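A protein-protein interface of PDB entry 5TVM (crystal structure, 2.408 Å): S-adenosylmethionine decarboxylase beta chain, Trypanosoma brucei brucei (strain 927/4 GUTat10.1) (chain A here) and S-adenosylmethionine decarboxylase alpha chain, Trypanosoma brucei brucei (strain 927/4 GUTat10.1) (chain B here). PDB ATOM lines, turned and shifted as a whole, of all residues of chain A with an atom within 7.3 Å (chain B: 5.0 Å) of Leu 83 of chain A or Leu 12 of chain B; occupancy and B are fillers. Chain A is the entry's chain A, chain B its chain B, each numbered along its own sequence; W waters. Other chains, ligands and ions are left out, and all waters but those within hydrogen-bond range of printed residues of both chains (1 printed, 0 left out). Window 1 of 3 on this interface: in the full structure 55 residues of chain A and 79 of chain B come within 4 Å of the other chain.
The backbone NH (N) of Lys 33 of chain A lies within hydrogen-bond range of the backbone carbonyl oxygen (O) of Thr 14 of chain B.
N of Leu 12 of chain B sits at hydrogen-bond distance from O of Leu 35 of chain A (2.8 Å).
The backbone carbonyl oxygen of Val 37 of chain A lies within hydrogen-bond range of the backbone NH of Val 10 of chain B (2.9 Å).
The backbone NH of Tyr 81 of chain A is in hydrogen-bond range of the backbone carbonyl oxygen of Leu 3 of chain B (2.9 Å).
N of Leu 83 of chain A sits at hydrogen-bond distance from O of PYR 1 of chain B (3.2 Å).
O of Leu 83 of chain A is in hydrogen-bond range of OH of Tyr 158 of chain B, at 3.3 Å.
The side-chain carboxylate of Glu 36 of chain A lies within salt-bridge range of the guanidinium group of Arg 34 of chain A (2.6 Å).
The backbone NH (N) of Ser 84 of chain A is in hydrogen-bond range of the backbone carbonyl oxygen (O) of His 68 of chain A, at 3.3 Å.
N of Val 70 of chain A lies within hydrogen-bond range of O of Val 82 of chain A (3.0 Å).
The backbone carbonyl oxygen (O) of Ser 71 of chain A is in hydrogen-bond range of the backbone NH (N) of Val 82 of chain A (3.3 Å).
The backbone NH (N) of Ser 2 of chain B sits at hydrogen-bond distance from the backbone carbonyl oxygen (O) of Ile 13 of chain B (2.8 Å).
The backbone carbonyl oxygen (O) of Leu 20 of chain B sits at hydrogen-bond distance from the side-chain sulfur (SG) of Cys 23 of chain B, at 3.4 Å.
CD2 of Leu 20 of chain B touches CB of Lys 33 of chain A, at 3.5 Å.
Leu 20 of chain B touches Arg 34 of chain A (CD2 to N, 3.8 Å).
O of Leu 35 of chain A touches CA of Ile 11 of chain B, at 3.4 Å.
Leu 20 of chain B touches Leu 35 of chain A (CD2 to CB, 3.7 Å).
Cys 23 of chain B touches Leu 35 of chain A.
Glu 36 of chain A touches Val 10 of chain B (CA to O, 3.2 Å).
Ile 27 of chain B touches Val 37 of chain A (CG2 to CG2, 3.7 Å).
Leu 3 of chain B touches Trp 58 of chain A (CD2 to CB, 3.9 Å).
Val 10 of chain B touches Trp 58 of chain A (CG2 to CH2, 3.7 Å).
Tyr 81 of chain A touches Ser 2 of chain B.
Leu 83 of chain A touches just these residues of chain B: PYR 1, Ser 2, Leu 12 and Tyr 158.
Leu 12 of chain B touches just these residues of chain A: Lys 33, Arg 34, Leu 35 and Leu 83.
Of the printed residues of chain A, Leu 20 of chain B touches Lys 33 (3.5 Å), Arg 34 (3.8 Å), Leu 35 (3.7 Å) and Ile 65 (3.8 Å).
Of the printed residues of chain A, Val 10 of chain B touches Leu 35, Glu 36, Val 37 and Trp 58.
Of the printed residues of chain B, Val 61 of chain A touches Cys 23.
Of the printed residues of chain A, Ile 11 of chain B touches Arg 34, Leu 35 and Glu 36.
The nearest printed residue of chain A that does not touch PYR 1 of chain B is Tyr 81 of chain A (4.4 Å).
Of the 12 printed residues of chain B, 12 touch a printed residue of chain A.
Printed residues of chain B that touch a printed residue of chain A: PYR 1, Ser 2, Leu 3, Val 10, Ile 11, Leu 12, Ile 13, Thr 14, Leu 20, Cys 23, Ile 27 and Tyr 158.
Hydrophobic or aromatic side chains of chain B within 4 Å of the printed part of chain A: Leu 3, Val 10, Ile 11, Leu 12, Ile 13, Leu 20, Ile 27 and Tyr 158.
Among the printed residues, 29 pairs touch across the chains.
Among the printed residues, no Asp or Glu carboxylate lies within 4 Å of a Lys or Arg side-chain nitrogen of the other chain.
Water W1 bridges NZ of Lys 33 of chain A and OG1 of Thr 14 of chain B.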
ATOM      1  N   LYS A  33       7.827   7.951   9.796  1.00  0.00           N
ATOM      2  CA  LYS A  33       8.679   6.815   9.490  1.00  0.00           C
ATOM      3  C   LYS A  33       7.810   5.569   9.378  1.00  0.00           C
ATOM      4  O   LYS A  33       6.868   5.387  10.154  1.00  0.00           O
ATOM      5  CB  LYS A  33       9.741   6.619  10.572  1.00  0.00           C
ATOM      6  CG  LYS A  33      10.483   7.889  10.939  1.00  0.00           C
ATOM      7  CD  LYS A  33      11.439   7.655  12.093  1.00  0.00           C
ATOM      8  CE  LYS A  33      12.125   8.943  12.518  1.00  0.00           C
ATOM      9  NZ  LYS A  33      11.152   9.991  12.927  1.00  0.00           N
ATOM     10  N   ARG A  34       8.127   4.718   8.407  1.00  0.00           N
ATOM     11  CA  ARG A  34       7.334   3.528   8.131  1.00  0.00           C
ATOM     12  C   ARG A  34       8.252   2.318   8.112  1.00  0.00           C
ATOM     13  O   ARG A  34       9.233   2.291   7.362  1.00  0.00           O
ATOM     14  CB  ARG A  34       6.589   3.659   6.801  1.00  0.00           C
ATOM     15  CG  ARG A  34       5.636   2.512   6.524  1.00  0.00           C
ATOM     16  CD  ARG A  34       4.954   2.665   5.173  1.00  0.00           C
ATOM     17  NE  ARG A  34       3.874   1.696   5.009  1.00  0.00           N
ATOM     18  CZ  ARG A  34       4.034   0.458   4.551  1.00  0.00           C
ATOM     19  NH1 ARG A  34       5.235   0.018   4.203  1.00  0.00           N
ATOM     20  NH2 ARG A  34       2.984  -0.346   4.443  1.00  0.00           N
ATOM     21  N   LEU A  35       7.935   1.326   8.938  1.00  0.00           N
ATOM     22  CA  LEU A  35       8.665   0.067   8.984  1.00  0.00           C
ATOM     23  C   LEU A  35       7.698  -1.063   8.668  1.00  0.00           C
ATOM     24  O   LEU A  35       6.628  -1.157   9.279  1.00  0.00           O
ATOM     25  CB  LEU A  35       9.305  -0.149  10.359  1.00  0.00           C
ATOM     26  CG  LEU A  35      10.039  -1.475  10.569  1.00  0.00           C
ATOM     27  CD1 LEU A  35      11.254  -1.569   9.655  1.00  0.00           C
ATOM     28  CD2 LEU A  35      10.439  -1.639  12.029  1.00  0.00           C
ATOM     29  N   GLU A  36       8.070  -1.915   7.714  1.00  0.00           N
ATOM     30  CA  GLU A  36       7.235  -3.042   7.318  1.00  0.00           C
ATOM     31  C   GLU A  36       8.082  -4.304   7.261  1.00  0.00           C
ATOM     32  O   GLU A  36       9.161  -4.305   6.661  1.00  0.00           O
ATOM     33  CB  GLU A  36       6.566  -2.792   5.960  1.00  0.00           C
ATOM     34  CG  GLU A  36       5.596  -3.895   5.556  1.00  0.00           C
ATOM     35  CD  GLU A  36       4.807  -3.564   4.304  1.00  0.00           C
ATOM     36  OE1 GLU A  36       5.094  -2.529   3.667  1.00  0.00           O
ATOM     37  OE2 GLU A  36       3.896  -4.345   3.959  1.00  0.00           O
ATOM     38  N   VAL A  37       7.586  -5.372   7.879  1.00  0.00           N
ATOM     39  CA  VAL A  37       8.263  -6.664   7.906  1.00  0.00           C
ATOM     40  C   VAL A  37       7.256  -7.726   7.494  1.00  0.00           C
ATOM     41  O   VAL A  37       6.212  -7.873   8.139  1.00  0.00           O
ATOM     42  CB  VAL A  37       8.844  -6.983   9.294  1.00  0.00           C
ATOM     43  CG1 VAL A  37       9.526  -8.350   9.291  1.00  0.00           C
ATOM     44  CG2 VAL A  37       9.819  -5.893   9.727  1.00  0.00           C
ATOM     45  N   TRP A  58       2.830  -7.181  21.394  1.00  0.00           N
ATOM     46  CA  TRP A  58       2.977  -5.931  20.663  1.00  0.00           C
ATOM     47  C   TRP A  58       3.159  -4.733  21.582  1.00  0.00           C
ATOM     48  O   TRP A  58       3.746  -3.732  21.160  1.00  0.00           O
ATOM     49  CB  TRP A  58       1.768  -5.721  19.749  1.00  0.00           C
ATOM     50  CG  TRP A  58       1.551  -6.882  18.832  1.00  0.00           C
ATOM     51  CD1 TRP A  58       0.451  -7.686  18.772  1.00  0.00           C
ATOM     52  CD2 TRP A  58       2.473  -7.389  17.860  1.00  0.00           C
ATOM     53  NE1 TRP A  58       0.627  -8.655  17.813  1.00  0.00           N
ATOM     54  CE2 TRP A  58       1.862  -8.496  17.241  1.00  0.00           C
ATOM     55  CE3 TRP A  58       3.756  -7.010  17.452  1.00  0.00           C
ATOM     56  CZ2 TRP A  58       2.488  -9.227  16.233  1.00  0.00           C
ATOM     57  CZ3 TRP A  58       4.376  -7.738  16.451  1.00  0.00           C
ATOM     58  CH2 TRP A  58       3.741  -8.833  15.853  1.00  0.00           C
ATOM     59  N   GLN A  59       2.688  -4.810  22.828  1.00  0.00           N
ATOM     60  CA  GLN A  59       2.928  -3.719  23.767  1.00  0.00           C
ATOM     61  C   GLN A  59       4.411  -3.598  24.096  1.00  0.00           C
ATOM     62  O   GLN A  59       4.940  -2.485  24.201  1.00  0.00           O
ATOM     63  CB  GLN A  59       2.109  -3.931  25.041  1.00  0.00           C
ATOM     64  CG  GLN A  59       2.273  -2.825  26.079  1.00  0.00           C
ATOM     65  CD  GLN A  59       1.826  -1.469  25.568  1.00  0.00           C
ATOM     66  OE1 GLN A  59       1.118  -1.371  24.567  1.00  0.00           O
ATOM     67  NE2 GLN A  59       2.241  -0.411  26.255  1.00  0.00           N
ATOM     68  N   VAL A  61       6.796  -4.315  22.114  1.00  0.00           N
ATOM     69  CA  VAL A  61       7.415  -3.710  20.938  1.00  0.00           C
ATOM     70  C   VAL A  61       7.322  -2.191  21.017  1.00  0.00           C
ATOM     71  O   VAL A  61       8.301  -1.476  20.774  1.00  0.00           O
ATOM     72  CB  VAL A  61       6.760  -4.252  19.654  1.00  0.00           C
ATOM     73  CG1 VAL A  61       7.291  -3.533  18.422  1.00  0.00           C
ATOM     74  CG2 VAL A  61       6.998  -5.751  19.533  1.00  0.00           C
ATOM     75  N   ILE A  62       6.140  -1.676  21.362  1.00  0.00           N
ATOM     76  CA  ILE A  62       5.948  -0.231  21.415  1.00  0.00           C
ATOM     77  C   ILE A  62       6.791   0.388  22.522  1.00  0.00           C
ATOM     78  O   ILE A  62       7.245   1.532  22.398  1.00  0.00           O
ATOM     79  CB  ILE A  62       4.452   0.101  21.588  1.00  0.00           C
ATOM     80  CG1 ILE A  62       3.614  -0.569  20.494  1.00  0.00           C
ATOM     81  CG2 ILE A  62       4.229   1.601  21.553  1.00  0.00           C
ATOM     82  CD1 ILE A  62       4.054  -0.244  19.079  1.00  0.00           C
ATOM     83  N   ILE A  65      10.290   1.751  21.684  1.00  0.00           N
ATOM     84  CA  ILE A  65      10.395   3.056  21.044  1.00  0.00           C
ATOM     85  C   ILE A  65       9.852   4.164  21.935  1.00  0.00           C
ATOM     86  O   ILE A  65       9.673   5.295  21.472  1.00  0.00           O
ATOM     87  CB  ILE A  65       9.692   3.062  19.675  1.00  0.00           C
ATOM     88  CG1 ILE A  65       8.221   2.660  19.822  1.00  0.00           C
ATOM     89  CG2 ILE A  65      10.413   2.128  18.712  1.00  0.00           C
ATOM     90  CD1 ILE A  65       7.413   2.792  18.545  1.00  0.00           C
ATOM     91  N   ALA A  67       6.787   4.581  23.424  1.00  0.00           N
ATOM     92  CA  ALA A  67       5.434   4.975  23.055  1.00  0.00           C
ATOM     93  C   ALA A  67       4.471   4.053  23.793  1.00  0.00           C
ATOM     94  O   ALA A  67       4.882   3.228  24.616  1.00  0.00           O
ATOM     95  CB  ALA A  67       5.251   4.930  21.532  1.00  0.00           C
ATOM     96  N   HIS A  68       3.180   4.175  23.497  1.00  0.00           N
ATOM     97  CA  HIS A  68       2.192   3.338  24.161  1.00  0.00           C
ATOM     98  C   HIS A  68       0.925   3.277  23.323  1.00  0.00           C
ATOM     99  O   HIS A  68       0.629   4.191  22.549  1.00  0.00           O
ATOM    100  CB  HIS A  68       1.872   3.859  25.567  1.00  0.00           C
ATOM    101  CG  HIS A  68       1.310   5.245  25.584  1.00  0.00           C
ATOM    102  ND1 HIS A  68       2.098   6.367  25.728  1.00  0.00           N
ATOM    103  CD2 HIS A  68       0.036   5.693  25.476  1.00  0.00           C
ATOM    104  CE1 HIS A  68       1.335   7.445  25.707  1.00  0.00           C
ATOM    105  NE2 HIS A  68       0.080   7.064  25.555  1.00  0.00           N
ATOM    106  N   ILE A  69       0.185   2.180  23.490  1.00  0.00           N
ATOM    107  CA  ILE A  69      -1.107   2.030  22.836  1.00  0.00           C
ATOM    108  C   ILE A  69      -2.132   2.918  23.532  1.00  0.00           C
ATOM    109  O   ILE A  69      -2.066   3.152  24.747  1.00  0.00           O
ATOM    110  CB  ILE A  69      -1.550   0.554  22.854  1.00  0.00           C
ATOM    111  CG1 ILE A  69      -0.515  -0.323  22.141  1.00  0.00           C
ATOM    112  CG2 ILE A  69      -2.926   0.395  22.209  1.00  0.00           C
ATOM    113  CD1 ILE A  69      -0.769  -1.814  22.283  1.00  0.00           C
ATOM    114  N   VAL A  70      -3.094   3.420  22.755  1.00  0.00           N
ATOM    115  CA  VAL A  70      -4.195   4.212  23.282  1.00  0.00           C
ATOM    116  C   VAL A  70      -5.537   3.516  23.086  1.00  0.00           C
ATOM    117  O   VAL A  70      -6.419   3.607  23.946  1.00  0.00           O
ATOM    118  CB  VAL A  70      -4.222   5.622  22.652  1.00  0.00           C
ATOM    119  CG1 VAL A  70      -2.886   6.322  22.865  1.00  0.00           C
ATOM    120  CG2 VAL A  70      -4.564   5.556  21.167  1.00  0.00           C
ATOM    121  N   SER A  71      -5.711   2.814  21.968  1.00  0.00           N
ATOM    122  CA  SER A  71      -6.938   2.082  21.699  1.00  0.00           C
ATOM    123  C   SER A  71      -6.626   0.940  20.746  1.00  0.00           C
ATOM    124  O   SER A  71      -5.678   1.009  19.958  1.00  0.00           O
ATOM    125  CB  SER A  71      -8.024   2.992  21.113  1.00  0.00           C
ATOM    126  OG  SER A  71      -7.577   3.635  19.934  1.00  0.00           O
ATOM    127  N   TYR A  81      -3.704  -0.819  16.075  1.00  0.00           N
ATOM    128  CA  TYR A  81      -3.366  -0.113  17.303  1.00  0.00           C
ATOM    129  C   TYR A  81      -3.063   1.339  16.967  1.00  0.00           C
ATOM    130  O   TYR A  81      -2.329   1.617  16.015  1.00  0.00           O
ATOM    131  CB  TYR A  81      -2.154  -0.748  18.000  1.00  0.00           C
ATOM    132  CG  TYR A  81      -2.270  -2.239  18.250  1.00  0.00           C
ATOM    133  CD1 TYR A  81      -1.945  -3.158  17.260  1.00  0.00           C
ATOM    134  CD2 TYR A  81      -2.683  -2.724  19.481  1.00  0.00           C
ATOM    135  CE1 TYR A  81      -2.041  -4.519  17.489  1.00  0.00           C
ATOM    136  CE2 TYR A  81      -2.783  -4.082  19.720  1.00  0.00           C
ATOM    137  CZ  TYR A  81      -2.461  -4.976  18.721  1.00  0.00           C
ATOM    138  OH  TYR A  81      -2.559  -6.328  18.956  1.00  0.00           O
ATOM    139  N   VAL A  82      -3.631   2.259  17.744  1.00  0.00           N
ATOM    140  CA  VAL A  82      -3.284   3.675  17.668  1.00  0.00           C
ATOM    141  C   VAL A  82      -2.254   3.958  18.748  1.00  0.00           C
ATOM    142  O   VAL A  82      -2.356   3.443  19.869  1.00  0.00           O
ATOM    143  CB  VAL A  82      -4.522   4.578  17.830  1.00  0.00           C
ATOM    144  CG1 VAL A  82      -4.124   6.049  17.833  1.00  0.00           C
ATOM    145  CG2 VAL A  82      -5.508   4.317  16.713  1.00  0.00           C
ATOM    146  N   LEU A  83      -1.260   4.776  18.413  1.00  0.00           N
ATOM    147  CA  LEU A  83      -0.124   5.016  19.289  1.00  0.00           C
ATOM    148  C   LEU A  83       0.051   6.511  19.506  1.00  0.00           C
ATOM    149  O   LEU A  83      -0.428   7.338  18.726  1.00  0.00           O
ATOM    150  CB  LEU A  83       1.161   4.417  18.702  1.00  0.00           C
ATOM    151  CG  LEU A  83       1.039   2.987  18.170  1.00  0.00           C
ATOM    152  CD1 LEU A  83       2.337   2.556  17.510  1.00  0.00           C
ATOM    153  CD2 LEU A  83       0.653   2.018  19.281  1.00  0.00           C
ATOM    154  N   SER A  84       0.746   6.848  20.590  1.00  0.00           N
ATOM    155  CA  SER A  84       1.056   8.234  20.901  1.00  0.00           C
ATOM    156  C   SER A  84       2.385   8.279  21.639  1.00  0.00           C
ATOM    157  O   SER A  84       2.736   7.349  22.370  1.00  0.00           O
ATOM    158  CB  SER A  84      -0.045   8.887  21.744  1.00  0.00           C
ATOM    159  OG  SER A  84       0.230  10.260  21.966  1.00  0.00           O
ATOM    160  N   GLU A  85       3.120   9.367  21.435  1.00  0.00           N
ATOM    161  CA  GLU A  85       4.417   9.543  22.077  1.00  0.00           C
ATOM    162  C   GLU A  85       4.290   9.454  23.594  1.00  0.00           C
ATOM    163  O   GLU A  85       3.208   9.634  24.152  1.00  0.00           O
ATOM    164  CB  GLU A  85       5.036  10.886  21.681  1.00  0.00           C
ATOM    165  CG  GLU A  85       5.424  10.982  20.214  1.00  0.00           C
ATOM    166  CD  GLU A  85       6.219  12.235  19.905  1.00  0.00           C
ATOM    167  OE1 GLU A  85       6.169  13.187  20.713  1.00  0.00           O
ATOM    168  OE2 GLU A  85       6.899  12.266  18.857  1.00  0.00           O
ATOM    169  OXT GLU A  85       5.267   9.198  24.298  1.00  0.00           O
ATOM    170  C   PYR B   1       0.412   5.547  14.959  1.00  0.00           C
ATOM    171  O   PYR B   1      -0.692   5.651  15.379  1.00  0.00           O
ATOM    172  CA  PYR B   1       1.440   6.641  15.229  1.00  0.00           C
ATOM    173  O3  PYR B   1       2.250   6.498  16.082  1.00  0.00           O
ATOM    174  CB  PYR B   1       1.428   7.921  14.396  1.00  0.00           C
ATOM    175  N   SER B   2       0.819   4.514  14.250  1.00  0.00           N
ATOM    176  CA  SER B   2      -0.039   3.383  13.921  1.00  0.00           C
ATOM    177  C   SER B   2       0.742   2.078  13.920  1.00  0.00           C
ATOM    178  O   SER B   2       1.923   2.047  13.574  1.00  0.00           O
ATOM    179  CB  SER B   2      -0.698   3.582  12.552  1.00  0.00           C
ATOM    180  OG  SER B   2      -1.611   4.660  12.570  1.00  0.00           O
ATOM    181  N   LEU B   3       0.067   1.001  14.310  1.00  0.00           N
ATOM    182  CA  LEU B   3       0.609  -0.348  14.218  1.00  0.00           C
ATOM    183  C   LEU B   3      -0.466  -1.250  13.639  1.00  0.00           C
ATOM    184  O   LEU B   3      -1.591  -1.287  14.148  1.00  0.00           O
ATOM    185  CB  LEU B   3       1.064  -0.871  15.589  1.00  0.00           C
ATOM    186  CG  LEU B   3       1.414  -2.362  15.675  1.00  0.00           C
ATOM    187  CD1 LEU B   3       2.657  -2.672  14.855  1.00  0.00           C
ATOM    188  CD2 LEU B   3       1.601  -2.798  17.123  1.00  0.00           C
ATOM    189  N   VAL B  10       3.977  -6.969   9.700  1.00  0.00           N
ATOM    190  CA  VAL B  10       3.794  -5.877  10.645  1.00  0.00           C
ATOM    191  C   VAL B  10       4.026  -4.579   9.890  1.00  0.00           C
ATOM    192  O   VAL B  10       4.890  -4.509   9.010  1.00  0.00           O
ATOM    193  CB  VAL B  10       4.754  -5.987  11.849  1.00  0.00           C
ATOM    194  CG1 VAL B  10       4.583  -4.798  12.787  1.00  0.00           C
ATOM    195  CG2 VAL B  10       4.524  -7.290  12.596  1.00  0.00           C
ATOM    196  N   ILE B  11       3.247  -3.556  10.223  1.00  0.00           N
ATOM    197  CA  ILE B  11       3.388  -2.231   9.634  1.00  0.00           C
ATOM    198  C   ILE B  11       3.369  -1.240  10.786  1.00  0.00           C
ATOM    199  O   ILE B  11       2.343  -1.082  11.457  1.00  0.00           O
ATOM    200  CB  ILE B  11       2.282  -1.918   8.616  1.00  0.00           C
ATOM    201  CG1 ILE B  11       2.432  -2.824   7.386  1.00  0.00           C
ATOM    202  CG2 ILE B  11       2.320  -0.439   8.209  1.00  0.00           C
ATOM    203  CD1 ILE B  11       1.291  -2.711   6.395  1.00  0.00           C
ATOM    204  N   LEU B  12       4.499  -0.580  11.020  1.00  0.00           N
ATOM    205  CA  LEU B  12       4.652   0.354  12.126  1.00  0.00           C
ATOM    206  C   LEU B  12       4.918   1.737  11.554  1.00  0.00           C
ATOM    207  O   LEU B  12       5.916   1.943  10.854  1.00  0.00           O
ATOM    208  CB  LEU B  12       5.786  -0.084  13.055  1.00  0.00           C
ATOM    209  CG  LEU B  12       6.079   0.804  14.266  1.00  0.00           C
ATOM    210  CD1 LEU B  12       4.814   1.117  15.050  1.00  0.00           C
ATOM    211  CD2 LEU B  12       7.107   0.131  15.167  1.00  0.00           C
ATOM    212  N   ILE B  13       4.021   2.675  11.843  1.00  0.00           N
ATOM    213  CA  ILE B  13       4.131   4.054  11.386  1.00  0.00           C
ATOM    214  C   ILE B  13       4.282   4.938  12.613  1.00  0.00           C
ATOM    215  O   ILE B  13       3.493   4.834  13.559  1.00  0.00           O
ATOM    216  CB  ILE B  13       2.906   4.478  10.553  1.00  0.00           C
ATOM    217  CG1 ILE B  13       2.767   3.579   9.320  1.00  0.00           C
ATOM    218  CG2 ILE B  13       3.021   5.945  10.139  1.00  0.00           C
ATOM    219  CD1 ILE B  13       1.472   3.776   8.552  1.00  0.00           C
ATOM    220  N   THR B  14       5.292   5.804  12.598  1.00  0.00           N
ATOM    221  CA  THR B  14       5.554   6.696  13.717  1.00  0.00           C
ATOM    222  C   THR B  14       5.912   8.076  13.186  1.00  0.00           C
ATOM    223  O   THR B  14       6.399   8.220  12.062  1.00  0.00           O
ATOM    224  CB  THR B  14       6.689   6.173  14.610  1.00  0.00           C
ATOM    225  OG1 THR B  14       7.910   6.130  13.861  1.00  0.00           O
ATOM    226  CG2 THR B  14       6.366   4.780  15.128  1.00  0.00           C
ATOM    227  N   LEU B  20      12.328   4.833  15.474  1.00  0.00           N
ATOM    228  CA  LEU B  20      11.535   3.686  15.048  1.00  0.00           C
ATOM    229  C   LEU B  20      12.357   2.404  14.973  1.00  0.00           C
ATOM    230  O   LEU B  20      11.829   1.317  15.226  1.00  0.00           O
ATOM    231  CB  LEU B  20      10.902   3.990  13.689  1.00  0.00           C
ATOM    232  CG  LEU B  20      10.193   2.836  12.986  1.00  0.00           C
ATOM    233  CD1 LEU B  20       9.117   2.261  13.878  1.00  0.00           C
ATOM    234  CD2 LEU B  20       9.596   3.306  11.671  1.00  0.00           C
ATOM    235  N   CYS B  23      12.895  -1.126  17.485  1.00  0.00           N
ATOM    236  CA  CYS B  23      11.983  -2.244  17.682  1.00  0.00           C
ATOM    237  C   CYS B  23      12.248  -3.406  16.733  1.00  0.00           C
ATOM    238  O   CYS B  23      11.510  -4.395  16.772  1.00  0.00           O
ATOM    239  CB  CYS B  23      10.537  -1.775  17.510  1.00  0.00           C
ATOM    240  SG  CYS B  23      10.032  -1.572  15.787  1.00  0.00           S
ATOM    241  N   ILE B  27      10.707  -7.389  16.638  1.00  0.00           N
ATOM    242  CA  ILE B  27       9.877  -7.846  15.529  1.00  0.00           C
ATOM    243  C   ILE B  27      10.436  -9.137  14.946  1.00  0.00           C
ATOM    244  O   ILE B  27       9.681 -10.058  14.610  1.00  0.00           O
ATOM    245  CB  ILE B  27       9.750  -6.741  14.463  1.00  0.00           C
ATOM    246  CG1 ILE B  27       8.826  -5.632  14.982  1.00  0.00           C
ATOM    247  CG2 ILE B  27       9.224  -7.314  13.141  1.00  0.00           C
ATOM    248  CD1 ILE B  27       8.674  -4.443  14.048  1.00  0.00           C
ATOM    249  N   TYR B 158      -6.323  15.103  19.850  1.00  0.00           N
ATOM    250  CA  TYR B 158      -5.282  15.429  20.812  1.00  0.00           C
ATOM    251  C   TYR B 158      -5.494  16.816  21.417  1.00  0.00           C
ATOM    252  O   TYR B 158      -6.350  17.595  20.989  1.00  0.00           O
ATOM    253  CB  TYR B 158      -3.906  15.352  20.152  1.00  0.00           C
ATOM    254  CG  TYR B 158      -3.457  13.949  19.812  1.00  0.00           C
ATOM    255  CD1 TYR B 158      -3.901  13.318  18.658  1.00  0.00           C
ATOM    256  CD2 TYR B 158      -2.577  13.263  20.637  1.00  0.00           C
ATOM    257  CE1 TYR B 158      -3.487  12.039  18.339  1.00  0.00           C
ATOM    258  CE2 TYR B 158      -2.156  11.984  20.327  1.00  0.00           C
ATOM    259  CZ  TYR B 158      -2.611  11.379  19.175  1.00  0.00           C
ATOM    260  OH  TYR B 158      -2.199  10.103  18.862  1.00  0.00           O
HETATM  261  O   HOH W   1       9.079   8.936  14.393  1.00  0.00           O
